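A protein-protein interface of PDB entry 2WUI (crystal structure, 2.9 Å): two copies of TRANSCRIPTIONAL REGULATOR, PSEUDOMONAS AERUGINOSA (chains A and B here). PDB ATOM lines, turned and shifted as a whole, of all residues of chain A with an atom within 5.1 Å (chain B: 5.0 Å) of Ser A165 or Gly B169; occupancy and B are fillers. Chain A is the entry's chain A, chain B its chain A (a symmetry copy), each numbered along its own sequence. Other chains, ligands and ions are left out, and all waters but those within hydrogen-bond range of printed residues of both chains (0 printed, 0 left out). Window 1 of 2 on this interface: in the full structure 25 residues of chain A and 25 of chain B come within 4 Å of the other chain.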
ATOM      1  N   SER A 160      15.553  26.222 -18.922  1.00  0.00           N
ATOM      2  CA  SER A 160      14.178  26.154 -18.469  1.00  0.00           C
ATOM      3  C   SER A 160      14.073  25.177 -17.304  1.00  0.00           C
ATOM      4  O   SER A 160      13.578  25.526 -16.228  1.00  0.00           O
ATOM      5  CB  SER A 160      13.250  25.732 -19.595  1.00  0.00           C
ATOM      6  OG  SER A 160      13.834  24.668 -20.305  1.00  0.00           O
ATOM      7  N   ILE A 161      14.554  23.955 -17.499  1.00  0.00           N
ATOM      8  CA  ILE A 161      14.460  22.980 -16.420  1.00  0.00           C
ATOM      9  C   ILE A 161      14.913  23.663 -15.129  1.00  0.00           C
ATOM     10  O   ILE A 161      14.309  23.468 -14.074  1.00  0.00           O
ATOM     11  CB  ILE A 161      15.276  21.699 -16.694  1.00  0.00           C
ATOM     12  CG1 ILE A 161      14.670  20.914 -17.858  1.00  0.00           C
ATOM     13  CG2 ILE A 161      15.300  20.823 -15.468  1.00  0.00           C
ATOM     14  CD1 ILE A 161      15.462  19.690 -18.238  1.00  0.00           C
ATOM     15  N   TYR A 162      15.934  24.507 -15.226  1.00  0.00           N
ATOM     16  CA  TYR A 162      16.424  25.231 -14.060  1.00  0.00           C
ATOM     17  C   TYR A 162      15.369  26.195 -13.516  1.00  0.00           C
ATOM     18  O   TYR A 162      14.973  26.091 -12.363  1.00  0.00           O
ATOM     19  CB  TYR A 162      17.730  25.967 -14.399  1.00  0.00           C
ATOM     20  CG  TYR A 162      18.383  26.667 -13.223  1.00  0.00           C
ATOM     21  CD1 TYR A 162      18.293  28.036 -13.069  1.00  0.00           C
ATOM     22  CD2 TYR A 162      19.110  25.956 -12.279  1.00  0.00           C
ATOM     23  CE1 TYR A 162      18.898  28.688 -11.995  1.00  0.00           C
ATOM     24  CE2 TYR A 162      19.722  26.599 -11.206  1.00  0.00           C
ATOM     25  CZ  TYR A 162      19.607  27.971 -11.070  1.00  0.00           C
ATOM     26  OH  TYR A 162      20.192  28.641 -10.014  1.00  0.00           O
ATOM     27  N   LEU A 163      14.908  27.131 -14.337  1.00  0.00           N
ATOM     28  CA  LEU A 163      13.875  28.078 -13.897  1.00  0.00           C
ATOM     29  C   LEU A 163      12.595  27.375 -13.415  1.00  0.00           C
ATOM     30  O   LEU A 163      12.083  27.643 -12.323  1.00  0.00           O
ATOM     31  CB  LEU A 163      13.551  29.071 -15.020  1.00  0.00           C
ATOM     32  CG  LEU A 163      13.967  30.536 -14.828  1.00  0.00           C
ATOM     33  CD1 LEU A 163      14.898  30.659 -13.642  1.00  0.00           C
ATOM     34  CD2 LEU A 163      14.616  31.111 -16.105  1.00  0.00           C
ATOM     35  N   GLN A 164      12.088  26.475 -14.250  1.00  0.00           N
ATOM     36  CA  GLN A 164      10.877  25.735 -13.958  1.00  0.00           C
ATOM     37  C   GLN A 164      11.017  24.993 -12.619  1.00  0.00           C
ATOM     38  O   GLN A 164      10.118  25.062 -11.782  1.00  0.00           O
ATOM     39  CB  GLN A 164      10.591  24.766 -15.097  1.00  0.00           C
ATOM     40  CG  GLN A 164       9.243  24.984 -15.725  1.00  0.00           C
ATOM     41  CD  GLN A 164       8.181  25.072 -14.677  1.00  0.00           C
ATOM     42  OE1 GLN A 164       7.494  26.105 -14.539  1.00  0.00           O
ATOM     43  NE2 GLN A 164       8.051  23.996 -13.889  1.00  0.00           N
ATOM     44  N   SER A 165      12.147  24.321 -12.384  1.00  0.00           N
ATOM     45  CA  SER A 165      12.394  23.747 -11.055  1.00  0.00           C
ATOM     46  C   SER A 165      12.313  24.803  -9.965  1.00  0.00           C
ATOM     47  O   SER A 165      11.599  24.642  -8.986  1.00  0.00           O
ATOM     48  CB  SER A 165      13.759  23.059 -10.975  1.00  0.00           C
ATOM     49  OG  SER A 165      13.755  21.826 -11.676  1.00  0.00           O
ATOM     50  N   LEU A 166      13.055  25.889 -10.132  1.00  0.00           N
ATOM     51  CA  LEU A 166      13.164  26.867  -9.057  1.00  0.00           C
ATOM     52  C   LEU A 166      11.771  27.338  -8.666  1.00  0.00           C
ATOM     53  O   LEU A 166      11.425  27.365  -7.491  1.00  0.00           O
ATOM     54  CB  LEU A 166      14.062  28.047  -9.465  1.00  0.00           C
ATOM     55  CG  LEU A 166      14.579  29.014  -8.386  1.00  0.00           C
ATOM     56  CD1 LEU A 166      15.454  30.139  -8.963  1.00  0.00           C
ATOM     57  CD2 LEU A 166      13.423  29.627  -7.636  1.00  0.00           C
ATOM     58  N   TRP A 167      10.981  27.726  -9.658  1.00  0.00           N
ATOM     59  CA  TRP A 167       9.604  28.128  -9.426  1.00  0.00           C
ATOM     60  C   TRP A 167       8.903  27.118  -8.517  1.00  0.00           C
ATOM     61  O   TRP A 167       8.618  27.407  -7.345  1.00  0.00           O
ATOM     62  CB  TRP A 167       8.881  28.197 -10.765  1.00  0.00           C
ATOM     63  CG  TRP A 167       7.729  29.116 -10.795  1.00  0.00           C
ATOM     64  CD1 TRP A 167       7.745  30.442 -11.114  1.00  0.00           C
ATOM     65  CD2 TRP A 167       6.376  28.780 -10.535  1.00  0.00           C
ATOM     66  NE1 TRP A 167       6.477  30.964 -11.049  1.00  0.00           N
ATOM     67  CE2 TRP A 167       5.609  29.959 -10.696  1.00  0.00           C
ATOM     68  CE3 TRP A 167       5.724  27.599 -10.162  1.00  0.00           C
ATOM     69  CZ2 TRP A 167       4.232  29.994 -10.498  1.00  0.00           C
ATOM     70  CZ3 TRP A 167       4.349  27.634  -9.965  1.00  0.00           C
ATOM     71  CH2 TRP A 167       3.620  28.825 -10.132  1.00  0.00           C
ATOM     72  N   ASP A 168       8.644  25.928  -9.066  1.00  0.00           N
ATOM     73  CA  ASP A 168       8.027  24.833  -8.315  1.00  0.00           C
ATOM     74  C   ASP A 168       8.533  24.708  -6.876  1.00  0.00           C
ATOM     75  O   ASP A 168       7.746  24.673  -5.927  1.00  0.00           O
ATOM     76  CB  ASP A 168       8.310  23.495  -8.996  1.00  0.00           C
ATOM     77  CG  ASP A 168       7.741  23.427 -10.421  1.00  0.00           C
ATOM     78  OD1 ASP A 168       7.258  24.473 -10.913  1.00  0.00           O
ATOM     79  OD2 ASP A 168       7.771  22.343 -11.056  1.00  0.00           O
ATOM     80  N   GLY A 169       9.848  24.633  -6.722  1.00  0.00           N
ATOM     81  CA  GLY A 169      10.494  24.779  -5.426  1.00  0.00           C
ATOM     82  C   GLY A 169       9.961  25.856  -4.481  1.00  0.00           C
ATOM     83  O   GLY A 169       9.641  25.537  -3.337  1.00  0.00           O
ATOM     84  N   ILE A 170       9.885  27.121  -4.906  1.00  0.00           N
ATOM     85  CA  ILE A 170       9.369  28.147  -3.992  1.00  0.00           C
ATOM     86  C   ILE A 170       7.849  28.043  -3.858  1.00  0.00           C
ATOM     87  O   ILE A 170       7.291  28.301  -2.788  1.00  0.00           O
ATOM     88  CB  ILE A 170       9.823  29.605  -4.344  1.00  0.00           C
ATOM     89  CG1 ILE A 170       9.107  30.132  -5.578  1.00  0.00           C
ATOM     90  CG2 ILE A 170      11.346  29.664  -4.579  1.00  0.00           C
ATOM     91  CD1 ILE A 170       9.991  30.030  -6.826  1.00  0.00           C
ATOM     92  N   SER B 165      14.610  25.069  -2.329  1.00  0.00           N
ATOM     93  CA  SER B 165      13.658  25.113  -3.446  1.00  0.00           C
ATOM     94  C   SER B 165      14.204  24.405  -4.675  1.00  0.00           C
ATOM     95  O   SER B 165      13.551  23.541  -5.243  1.00  0.00           O
ATOM     96  CB  SER B 165      13.289  26.549  -3.825  1.00  0.00           C
ATOM     97  OG  SER B 165      12.424  27.129  -2.862  1.00  0.00           O
ATOM     98  N   LEU B 166      15.405  24.779  -5.093  1.00  0.00           N
ATOM     99  CA  LEU B 166      15.924  24.273  -6.357  1.00  0.00           C
ATOM    100  C   LEU B 166      15.919  22.752  -6.328  1.00  0.00           C
ATOM    101  O   LEU B 166      15.444  22.108  -7.256  1.00  0.00           O
ATOM    102  CB  LEU B 166      17.331  24.825  -6.643  1.00  0.00           C
ATOM    103  CG  LEU B 166      17.925  24.692  -8.056  1.00  0.00           C
ATOM    104  CD1 LEU B 166      19.338  25.285  -8.168  1.00  0.00           C
ATOM    105  CD2 LEU B 166      17.968  23.242  -8.471  1.00  0.00           C
ATOM    106  N   TRP B 167      16.468  22.183  -5.263  1.00  0.00           N
ATOM    107  CA  TRP B 167      16.461  20.740  -5.078  1.00  0.00           C
ATOM    108  C   TRP B 167      15.067  20.178  -5.357  1.00  0.00           C
ATOM    109  O   TRP B 167      14.843  19.508  -6.376  1.00  0.00           O
ATOM    110  CB  TRP B 167      16.860  20.429  -3.641  1.00  0.00           C
ATOM    111  CG  TRP B 167      17.464  19.098  -3.447  1.00  0.00           C
ATOM    112  CD1 TRP B 167      18.787  18.778  -3.531  1.00  0.00           C
ATOM    113  CD2 TRP B 167      16.783  17.906  -3.095  1.00  0.00           C
ATOM    114  NE1 TRP B 167      18.973  17.443  -3.270  1.00  0.00           N
ATOM    115  CE2 TRP B 167      17.751  16.879  -2.995  1.00  0.00           C
ATOM    116  CE3 TRP B 167      15.439  17.588  -2.867  1.00  0.00           C
ATOM    117  CZ2 TRP B 167      17.423  15.563  -2.680  1.00  0.00           C
ATOM    118  CZ3 TRP B 167      15.111  16.275  -2.552  1.00  0.00           C
ATOM    119  CH2 TRP B 167      16.101  15.280  -2.463  1.00  0.00           C
ATOM    120  N   ASP B 168      14.132  20.471  -4.448  1.00  0.00           N
ATOM    121  CA  ASP B 168      12.736  20.055  -4.594  1.00  0.00           C
ATOM    122  C   ASP B 168      12.204  20.160  -6.025  1.00  0.00           C
ATOM    123  O   ASP B 168      11.663  19.197  -6.575  1.00  0.00           O
ATOM    124  CB  ASP B 168      11.828  20.923  -3.725  1.00  0.00           C
ATOM    125  CG  ASP B 168      12.166  20.817  -2.230  1.00  0.00           C
ATOM    126  OD1 ASP B 168      13.193  20.180  -1.902  1.00  0.00           O
ATOM    127  OD2 ASP B 168      11.419  21.362  -1.379  1.00  0.00           O
ATOM    128  N   GLY B 169      12.355  21.336  -6.620  1.00  0.00           N
ATOM    129  CA  GLY B 169      12.151  21.522  -8.049  1.00  0.00           C
ATOM    130  C   GLY B 169      12.674  20.437  -8.991  1.00  0.00           C
ATOM    131  O   GLY B 169      11.902  19.936  -9.807  1.00  0.00           O
ATOM    132  N   ILE B 170      13.961  20.082  -8.931  1.00  0.00           N
ATOM    133  CA  ILE B 170      14.453  19.037  -9.837  1.00  0.00           C
ATOM    134  C   ILE B 170      13.992  17.653  -9.376  1.00  0.00           C
ATOM    135  O   ILE B 170      13.721  16.773 -10.196  1.00  0.00           O
ATOM    136  CB  ILE B 170      15.999  19.082 -10.088  1.00  0.00           C
ATOM    137  CG1 ILE B 170      16.778  18.601  -8.872  1.00  0.00           C
ATOM    138  CG2 ILE B 170      16.456  20.510 -10.448  1.00  0.00           C
ATOM    139  CD1 ILE B 170      17.323  19.776  -8.054  1.00  0.00           C
ATOM    140  N   CYS B 171      13.879  17.483  -8.062  1.00  0.00           N
ATOM    141  CA  CYS B 171      13.286  16.275  -7.506  1.00  0.00           C
ATOM    142  C   CYS B 171      11.965  15.990  -8.215  1.00  0.00           C
ATOM    143  O   CYS B 171      11.755  14.903  -8.739  1.00  0.00           O
ATOM    144  CB  CYS B 171      13.047  16.428  -6.003  1.00  0.00           C
ATOM    145  SG  CYS B 171      13.540  14.980  -5.035  1.00  0.00           S
ATOM    146  N   GLY B 172      11.086  16.977  -8.261  1.00  0.00           N
ATOM    147  CA  GLY B 172       9.828  16.815  -8.956  1.00  0.00           C
ATOM    148  C   GLY B 172       9.910  16.664 -10.466  1.00  0.00           C
ATOM    149  O   GLY B 172       8.907  16.365 -11.104  1.00  0.00           O
ATOM    150  N   THR B 173      11.075  16.883 -11.068  1.00  0.00           N
ATOM    151  CA  THR B 173      11.155  16.742 -12.525  1.00  0.00           C
ATOM    152  C   THR B 173      11.738  15.385 -12.905  1.00  0.00           C
ATOM    153  O   THR B 173      11.585  14.906 -14.034  1.00  0.00           O
ATOM    154  CB  THR B 173      11.963  17.879 -13.209  1.00  0.00           C
ATOM    155  OG1 THR B 173      13.357  17.708 -12.929  1.00  0.00           O
ATOM    156  CG2 THR B 173      11.490  19.280 -12.756  1.00  0.00           C
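The backbone NH (N) of Ile A170 lies close to the side-chain hydroxyl (OG) of Ser B165 (3.3 Å). OG of Ser A165 lies close to N of Ile B170 (3.3 Å). O of Gly A169 lies close to OG of Ser B165 (3.2 Å). OG of Ser A165 lies close to O of Gly B169 (3.2 Å).
The backbone carbonyl oxygen (O) of Ile B170 sits at hydrogen-bond distance from the side-chain hydroxyl (OG1) of Thr B173, 2.9 Å away. O of Ile A161 lies within hydrogen-bond range of OG of Ser A165, at 3.0 Å.
Leu B166 touches Tyr A162. CG2 of Thr B173 touches OG of Ser A165, 3.6 Å away.
Printed residues of chain B within 4 Å of Ser A165: Gly B169, Ile B170 and Thr B173. Leu A166 touches none of the printed residues of chain B. Of the printed residues of chain B, Gly A169 touches Ser B165. Asp B168 touches none of the printed residues of chain A. Gly B169 touches one residue of chain A. Printed residues of chain A within 4 Å of Thr B173: Ser A165 (3.6 Å). The nearest printed residue of chain B that does not touch Ile A170 is Leu B166 (6.0 Å).
Along chain B the printed residues that touch a printed residue of chain A span positions 165 to 173. Hydrophobic or aromatic side chains of chain A that line the printed part of chain B: Tyr A162 and Ile A170. Among the printed residues, 6 pairs touch across the chains. Among the printed residues, no Asp or Glu carboxylate lies within 4 Å of a Lys or Arg side-chain nitrogen of the other chain.
Ser A165 touches Gly B169, and with the chains exchanged Gly A169 touches Ser B165. Ser A165 touches Ile B170, and with the chains exchanged Ile A170 touches Ser B165. 6 positions are printed for both chains.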
